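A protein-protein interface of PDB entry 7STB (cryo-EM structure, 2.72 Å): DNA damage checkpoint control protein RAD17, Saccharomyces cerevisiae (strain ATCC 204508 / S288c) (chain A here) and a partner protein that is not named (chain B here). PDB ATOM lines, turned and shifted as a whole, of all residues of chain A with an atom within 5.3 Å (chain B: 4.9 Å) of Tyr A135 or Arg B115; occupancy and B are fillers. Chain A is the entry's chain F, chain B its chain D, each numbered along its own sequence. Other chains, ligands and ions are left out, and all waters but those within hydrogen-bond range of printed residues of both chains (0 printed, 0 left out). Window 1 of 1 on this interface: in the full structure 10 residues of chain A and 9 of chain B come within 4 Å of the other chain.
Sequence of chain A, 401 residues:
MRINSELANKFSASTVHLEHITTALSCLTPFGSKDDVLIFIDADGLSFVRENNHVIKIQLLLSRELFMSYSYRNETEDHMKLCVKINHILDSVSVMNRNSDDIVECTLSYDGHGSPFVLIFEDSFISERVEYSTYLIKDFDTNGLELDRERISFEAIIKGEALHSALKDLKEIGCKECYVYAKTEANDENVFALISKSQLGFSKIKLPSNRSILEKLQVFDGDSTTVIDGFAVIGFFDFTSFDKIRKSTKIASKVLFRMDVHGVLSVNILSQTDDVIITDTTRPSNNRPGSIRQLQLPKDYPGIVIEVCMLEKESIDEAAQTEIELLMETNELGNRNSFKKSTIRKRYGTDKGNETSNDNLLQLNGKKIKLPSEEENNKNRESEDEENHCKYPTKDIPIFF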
ATOM      1  N   ASP A  36      36.736 -22.642  19.773  1.00  0.00           N
ATOM      2  CA  ASP A  36      36.347 -22.494  21.166  1.00  0.00           C
ATOM      3  C   ASP A  36      36.859 -23.683  21.968  1.00  0.00           C
ATOM      4  O   ASP A  36      37.126 -24.757  21.424  1.00  0.00           O
ATOM      5  CB  ASP A  36      34.825 -22.382  21.312  1.00  0.00           C
ATOM      6  CG  ASP A  36      34.102 -23.631  20.850  1.00  0.00           C
ATOM      7  OD1 ASP A  36      34.683 -24.395  20.052  1.00  0.00           O
ATOM      8  OD2 ASP A  36      32.953 -23.851  21.285  1.00  0.00           O
ATOM      9  N   CYS A  83      32.108 -22.758  28.082  1.00  0.00           N
ATOM     10  CA  CYS A  83      32.774 -22.550  26.803  1.00  0.00           C
ATOM     11  C   CYS A  83      33.484 -21.205  26.808  1.00  0.00           C
ATOM     12  O   CYS A  83      32.939 -20.211  27.298  1.00  0.00           O
ATOM     13  CB  CYS A  83      31.771 -22.612  25.646  1.00  0.00           C
ATOM     14  SG  CYS A  83      32.515 -22.523  24.007  1.00  0.00           S
ATOM     15  N   VAL A  84      34.698 -21.175  26.260  1.00  0.00           N
ATOM     16  CA  VAL A  84      35.524 -19.974  26.237  1.00  0.00           C
ATOM     17  C   VAL A  84      36.124 -19.812  24.848  1.00  0.00           C
ATOM     18  O   VAL A  84      36.547 -20.792  24.225  1.00  0.00           O
ATOM     19  CB  VAL A  84      36.636 -20.034  27.306  1.00  0.00           C
ATOM     20  CG1 VAL A  84      37.594 -18.864  27.148  1.00  0.00           C
ATOM     21  CG2 VAL A  84      36.031 -20.047  28.699  1.00  0.00           C
ATOM     22  N   LYS A  85      36.168 -18.575  24.363  1.00  0.00           N
ATOM     23  CA  LYS A  85      36.748 -18.300  23.055  1.00  0.00           C
ATOM     24  C   LYS A  85      38.261 -18.176  23.168  1.00  0.00           C
ATOM     25  O   LYS A  85      38.776 -17.474  24.045  1.00  0.00           O
ATOM     26  CB  LYS A  85      36.149 -17.030  22.453  1.00  0.00           C
ATOM     27  CG  LYS A  85      34.885 -17.283  21.646  1.00  0.00           C
ATOM     28  CD  LYS A  85      34.351 -16.010  21.015  1.00  0.00           C
ATOM     29  CE  LYS A  85      32.985 -16.239  20.385  1.00  0.00           C
ATOM     30  NZ  LYS A  85      33.062 -17.112  19.184  1.00  0.00           N
ATOM     31  N   ASN A  87      40.941 -16.545  21.974  1.00  0.00           N
ATOM     32  CA  ASN A  87      41.548 -15.421  21.261  1.00  0.00           C
ATOM     33  C   ASN A  87      43.059 -15.410  21.475  1.00  0.00           C
ATOM     34  O   ASN A  87      43.835 -15.587  20.530  1.00  0.00           O
ATOM     35  CB  ASN A  87      40.915 -14.102  21.715  1.00  0.00           C
ATOM     36  CG  ASN A  87      39.474 -13.967  21.270  1.00  0.00           C
ATOM     37  OD1 ASN A  87      38.560 -13.932  22.092  1.00  0.00           O
ATOM     38  ND2 ASN A  87      39.263 -13.889  19.962  1.00  0.00           N
ATOM     39  N   SER A 133      34.589 -14.353  29.380  1.00  0.00           N
ATOM     40  CA  SER A 133      33.151 -14.536  29.267  1.00  0.00           C
ATOM     41  C   SER A 133      32.831 -15.917  28.708  1.00  0.00           C
ATOM     42  O   SER A 133      33.591 -16.484  27.917  1.00  0.00           O
ATOM     43  CB  SER A 133      32.542 -13.456  28.374  1.00  0.00           C
ATOM     44  OG  SER A 133      32.892 -12.161  28.830  1.00  0.00           O
ATOM     45  N   THR A 134      31.694 -16.459  29.133  1.00  0.00           N
ATOM     46  CA  THR A 134      31.240 -17.764  28.681  1.00  0.00           C
ATOM     47  C   THR A 134      30.258 -17.618  27.522  1.00  0.00           C
ATOM     48  O   THR A 134      29.723 -16.539  27.260  1.00  0.00           O
ATOM     49  CB  THR A 134      30.587 -18.536  29.828  1.00  0.00           C
ATOM     50  OG1 THR A 134      29.445 -17.815  30.306  1.00  0.00           O
ATOM     51  CG2 THR A 134      31.573 -18.738  30.969  1.00  0.00           C
ATOM     52  N   TYR A 135      30.023 -18.732  26.828  1.00  0.00           N
ATOM     53  CA  TYR A 135      29.171 -18.755  25.649  1.00  0.00           C
ATOM     54  C   TYR A 135      28.221 -19.940  25.705  1.00  0.00           C
ATOM     55  O   TYR A 135      28.472 -20.931  26.396  1.00  0.00           O
ATOM     56  CB  TYR A 135      29.992 -18.827  24.357  1.00  0.00           C
ATOM     57  CG  TYR A 135      31.122 -17.835  24.309  1.00  0.00           C
ATOM     58  CD1 TYR A 135      31.001 -16.655  23.591  1.00  0.00           C
ATOM     59  CD2 TYR A 135      32.310 -18.076  24.980  1.00  0.00           C
ATOM     60  CE1 TYR A 135      32.028 -15.743  23.547  1.00  0.00           C
ATOM     61  CE2 TYR A 135      33.342 -17.172  24.940  1.00  0.00           C
ATOM     62  CZ  TYR A 135      33.195 -16.008  24.222  1.00  0.00           C
ATOM     63  OH  TYR A 135      34.224 -15.106  24.180  1.00  0.00           O
ATOM     64  N   LEU A 136      27.119 -19.817  24.969  1.00  0.00           N
ATOM     65  CA  LEU A 136      26.149 -20.897  24.878  1.00  0.00           C
ATOM     66  C   LEU A 136      26.824 -22.155  24.345  1.00  0.00           C
ATOM     67  O   LEU A 136      27.558 -22.110  23.354  1.00  0.00           O
ATOM     68  CB  LEU A 136      24.992 -20.470  23.971  1.00  0.00           C
ATOM     69  CG  LEU A 136      23.762 -21.373  23.859  1.00  0.00           C
ATOM     70  CD1 LEU A 136      22.543 -20.543  23.504  1.00  0.00           C
ATOM     71  CD2 LEU A 136      23.968 -22.453  22.813  1.00  0.00           C
ATOM     72  N   ILE A 137      26.576 -23.282  25.012  1.00  0.00           N
ATOM     73  CA  ILE A 137      27.226 -24.535  24.644  1.00  0.00           C
ATOM     74  C   ILE A 137      26.718 -24.972  23.277  1.00  0.00           C
ATOM     75  O   ILE A 137      25.512 -25.153  23.074  1.00  0.00           O
ATOM     76  CB  ILE A 137      26.972 -25.617  25.702  1.00  0.00           C
ATOM     77  CG1 ILE A 137      27.539 -25.190  27.061  1.00  0.00           C
ATOM     78  CG2 ILE A 137      27.577 -26.943  25.262  1.00  0.00           C
ATOM     79  CD1 ILE A 137      29.049 -25.026  27.089  1.00  0.00           C
ATOM     80  N   LYS A 138      27.641 -25.162  22.338  1.00  0.00           N
ATOM     81  CA  LYS A 138      27.261 -25.543  20.985  1.00  0.00           C
ATOM     82  C   LYS A 138      26.446 -26.829  21.004  1.00  0.00           C
ATOM     83  O   LYS A 138      26.765 -27.778  21.726  1.00  0.00           O
ATOM     84  CB  LYS A 138      28.507 -25.728  20.118  1.00  0.00           C
ATOM     85  CG  LYS A 138      29.036 -24.444  19.500  1.00  0.00           C
ATOM     86  CD  LYS A 138      28.125 -23.926  18.399  1.00  0.00           C
ATOM     87  CE  LYS A 138      28.747 -22.741  17.678  1.00  0.00           C
ATOM     88  NZ  LYS A 138      27.785 -22.072  16.762  1.00  0.00           N
ATOM     89  N   LYS B 111      27.578 -11.637  16.078  1.00  0.00           N
ATOM     90  CA  LYS B 111      27.515 -13.066  16.364  1.00  0.00           C
ATOM     91  C   LYS B 111      28.118 -13.383  17.726  1.00  0.00           C
ATOM     92  O   LYS B 111      27.546 -14.162  18.500  1.00  0.00           O
ATOM     93  CB  LYS B 111      28.232 -13.849  15.264  1.00  0.00           C
ATOM     94  CG  LYS B 111      28.145 -15.358  15.421  1.00  0.00           C
ATOM     95  CD  LYS B 111      28.778 -16.076  14.241  1.00  0.00           C
ATOM     96  CE  LYS B 111      27.823 -16.165  13.064  1.00  0.00           C
ATOM     97  NZ  LYS B 111      26.670 -17.064  13.342  1.00  0.00           N
ATOM     98  N   ASN B 112      29.269 -12.783  18.044  1.00  0.00           N
ATOM     99  CA  ASN B 112      29.901 -13.042  19.331  1.00  0.00           C
ATOM    100  C   ASN B 112      29.017 -12.580  20.479  1.00  0.00           C
ATOM    101  O   ASN B 112      28.877 -13.284  21.487  1.00  0.00           O
ATOM    102  CB  ASN B 112      31.263 -12.351  19.390  1.00  0.00           C
ATOM    103  CG  ASN B 112      32.287 -13.005  18.485  1.00  0.00           C
ATOM    104  OD1 ASN B 112      32.129 -14.155  18.078  1.00  0.00           O
ATOM    105  ND2 ASN B 112      33.346 -12.271  18.162  1.00  0.00           N
ATOM    106  N   PHE B 113      28.410 -11.398  20.351  1.00  0.00           N
ATOM    107  CA  PHE B 113      27.529 -10.920  21.410  1.00  0.00           C
ATOM    108  C   PHE B 113      26.298 -11.807  21.548  1.00  0.00           C
ATOM    109  O   PHE B 113      25.864 -12.105  22.667  1.00  0.00           O
ATOM    110  CB  PHE B 113      27.115  -9.474  21.151  1.00  0.00           C
ATOM    111  CG  PHE B 113      26.447  -8.823  22.326  1.00  0.00           C
ATOM    112  CD1 PHE B 113      27.184  -8.441  23.433  1.00  0.00           C
ATOM    113  CD2 PHE B 113      25.080  -8.604  22.330  1.00  0.00           C
ATOM    114  CE1 PHE B 113      26.572  -7.848  24.519  1.00  0.00           C
ATOM    115  CE2 PHE B 113      24.464  -8.011  23.414  1.00  0.00           C
ATOM    116  CZ  PHE B 113      25.211  -7.632  24.508  1.00  0.00           C
ATOM    117  N   ALA B 114      25.720 -12.239  20.424  1.00  0.00           N
ATOM    118  CA  ALA B 114      24.530 -13.079  20.485  1.00  0.00           C
ATOM    119  C   ALA B 114      24.835 -14.419  21.139  1.00  0.00           C
ATOM    120  O   ALA B 114      24.022 -14.940  21.911  1.00  0.00           O
ATOM    121  CB  ALA B 114      23.962 -13.282  19.081  1.00  0.00           C
ATOM    122  N   ARG B 115      26.001 -14.994  20.843  1.00  0.00           N
ATOM    123  CA  ARG B 115      26.376 -16.281  21.414  1.00  0.00           C
ATOM    124  C   ARG B 115      26.783 -16.193  22.881  1.00  0.00           C
ATOM    125  O   ARG B 115      26.903 -17.234  23.535  1.00  0.00           O
ATOM    126  CB  ARG B 115      27.520 -16.894  20.602  1.00  0.00           C
ATOM    127  CG  ARG B 115      27.706 -18.387  20.810  1.00  0.00           C
ATOM    128  CD  ARG B 115      28.919 -18.903  20.057  1.00  0.00           C
ATOM    129  NE  ARG B 115      29.366 -20.198  20.557  1.00  0.00           N
ATOM    130  CZ  ARG B 115      30.536 -20.751  20.266  1.00  0.00           C
ATOM    131  NH1 ARG B 115      31.408 -20.148  19.472  1.00  0.00           N
ATOM    132  NH2 ARG B 115      30.841 -21.936  20.785  1.00  0.00           N
ATOM    133  N   LEU B 116      26.992 -14.992  23.413  1.00  0.00           N
ATOM    134  CA  LEU B 116      27.423 -14.846  24.796  1.00  0.00           C
ATOM    135  C   LEU B 116      26.323 -15.281  25.758  1.00  0.00           C
ATOM    136  O   LEU B 116      25.129 -15.165  25.469  1.00  0.00           O
ATOM    137  CB  LEU B 116      27.812 -13.396  25.087  1.00  0.00           C
ATOM    138  CG  LEU B 116      29.285 -13.021  24.921  1.00  0.00           C
ATOM    139  CD1 LEU B 116      29.456 -11.515  25.025  1.00  0.00           C
ATOM    140  CD2 LEU B 116      30.149 -13.729  25.950  1.00  0.00           C
ATOM    141  N   THR B 117      26.739 -15.787  26.917  1.00  0.00           N
ATOM    142  CA  THR B 117      25.801 -16.116  27.980  1.00  0.00           C
ATOM    143  C   THR B 117      25.378 -14.852  28.715  1.00  0.00           C
ATOM    144  O   THR B 117      26.187 -13.949  28.946  1.00  0.00           O
ATOM    145  CB  THR B 117      26.421 -17.099  28.972  1.00  0.00           C
ATOM    146  OG1 THR B 117      27.574 -16.505  29.581  1.00  0.00           O
ATOM    147  CG2 THR B 117      26.820 -18.384  28.277  1.00  0.00           C
ATOM    148  N   LYS B 135      19.516 -11.316  26.340  1.00  0.00           N
ATOM    149  CA  LYS B 135      19.990  -9.963  26.103  1.00  0.00           C
ATOM    150  C   LYS B 135      19.296  -9.384  24.870  1.00  0.00           C
ATOM    151  O   LYS B 135      18.445 -10.023  24.247  1.00  0.00           O
ATOM    152  CB  LYS B 135      21.511  -9.949  25.940  1.00  0.00           C
ATOM    153  CG  LYS B 135      22.002 -10.565  24.642  1.00  0.00           C
ATOM    154  CD  LYS B 135      23.479 -10.917  24.717  1.00  0.00           C
ATOM    155  CE  LYS B 135      23.704 -12.262  25.384  1.00  0.00           C
ATOM    156  NZ  LYS B 135      23.281 -13.392  24.513  1.00  0.00           N
ATOM    157  N   TYR B 160      20.718 -18.383  17.950  1.00  0.00           N
ATOM    158  CA  TYR B 160      20.911 -17.939  19.327  1.00  0.00           C
ATOM    159  C   TYR B 160      19.691 -17.190  19.853  1.00  0.00           C
ATOM    160  O   TYR B 160      19.812 -16.241  20.629  1.00  0.00           O
ATOM    161  CB  TYR B 160      22.158 -17.065  19.436  1.00  0.00           C
ATOM    162  CG  TYR B 160      23.357 -17.632  18.712  1.00  0.00           C
ATOM    163  CD1 TYR B 160      23.973 -18.793  19.154  1.00  0.00           C
ATOM    164  CD2 TYR B 160      23.872 -17.004  17.587  1.00  0.00           C
ATOM    165  CE1 TYR B 160      25.068 -19.315  18.496  1.00  0.00           C
ATOM    166  CE2 TYR B 160      24.967 -17.518  16.923  1.00  0.00           C
ATOM    167  CZ  TYR B 160      25.561 -18.673  17.381  1.00  0.00           C
ATOM    168  OH  TYR B 160      26.652 -19.188  16.721  1.00  0.00           O
ATOM    169  N   THR B 164      19.350 -14.470  23.030  1.00  0.00           N
ATOM    170  CA  THR B 164      19.483 -13.163  22.405  1.00  0.00           C
ATOM    171  C   THR B 164      18.190 -12.802  21.689  1.00  0.00           C
ATOM    172  O   THR B 164      17.483 -13.670  21.172  1.00  0.00           O
ATOM    173  CB  THR B 164      20.648 -13.132  21.406  1.00  0.00           C
ATOM    174  OG1 THR B 164      21.832 -13.637  22.034  1.00  0.00           O
ATOM    175  CG2 THR B 164      20.903 -11.713  20.925  1.00  0.00           C
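OD1 of Asn B112 sits close to NZ of Lys A85. NH2 of Arg B115 is in salt-bridge range of OD2 of Asp A36 (2.9 Å). The side-chain sulfur (SG) of Cys A83 lies within hydrogen-bond range of the guanidinium group (NH2) of Arg B115, at 3.7 Å. The backbone NH of Leu A136 lies within hydrogen-bond range of the backbone carbonyl oxygen of Arg B115 (3.0 Å). N of Thr B117 sits at hydrogen-bond distance from O of Thr A134 (3.1 Å). NZ of Lys A138 is in hydrogen-bond range of OH of Tyr B160. The guanidinium group (NH1) of Arg B115 lies close to the side-chain amino group (NZ) of Lys A85.
NZ of Lys B135 lies within hydrogen-bond range of O of Leu B116 (2.7 Å). OD2 of Asp A36 lies within hydrogen-bond range of SG of Cys A83 (3.1 Å). O of Cys A83 sits close to N of Tyr A135 (3.3 Å).
Ser A133 touches Leu B116 (CB to CD2, 3.4 Å). Thr A134 touches Leu B116 (O to CD2, 3.1 Å). Arg B115 touches Tyr A135. Tyr A135 touches Leu B116. CG2 of Thr B117 touches C of Tyr A135, at 3.3 Å. Leu A136 touches Thr B117. Lys A138 touches Arg B115.
Asn A87 touches none of the printed residues of chain B. Printed residues of chain B within 4 Å of Ser A133: Leu B116. Of the printed residues of chain B, Thr A134 touches Leu B116 and Thr B117. Of chain B, only Arg B115, Leu B116 and Thr B117 come within 4 Å of Tyr A135. Printed residues of chain B within 4 Å of Leu A136: Arg B115 and Thr B117. Lys B111 touches none of the printed residues of chain A. Of the printed residues of chain A, Thr B117 touches Thr A134 (2.4 Å), Tyr A135 (3.3 Å) and Leu A136 (3.6 Å). Of the printed residues of chain A, Tyr B160 touches Lys A138. The nearest residue of chain A that does not touch Arg B115 is Thr A134 (4.7 Å). The nearest printed residue of chain B that does not touch Cys A83 is Thr B117 (6.5 Å).
Of the 11 printed residues of chain A, 8 touch a printed residue of chain B. Hydrophobic or aromatic side chains of chain A that line the printed part of chain B: Tyr A135 and Leu A136. Of the 10 printed residues of chain B, 5 touch a printed residue of chain A. Hydrophobic or aromatic side chains of chain B that line the printed part of chain A: Leu B116 and Tyr B160. Along chain B the printed residues that touch a printed residue of chain A span positions 112 to 160.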
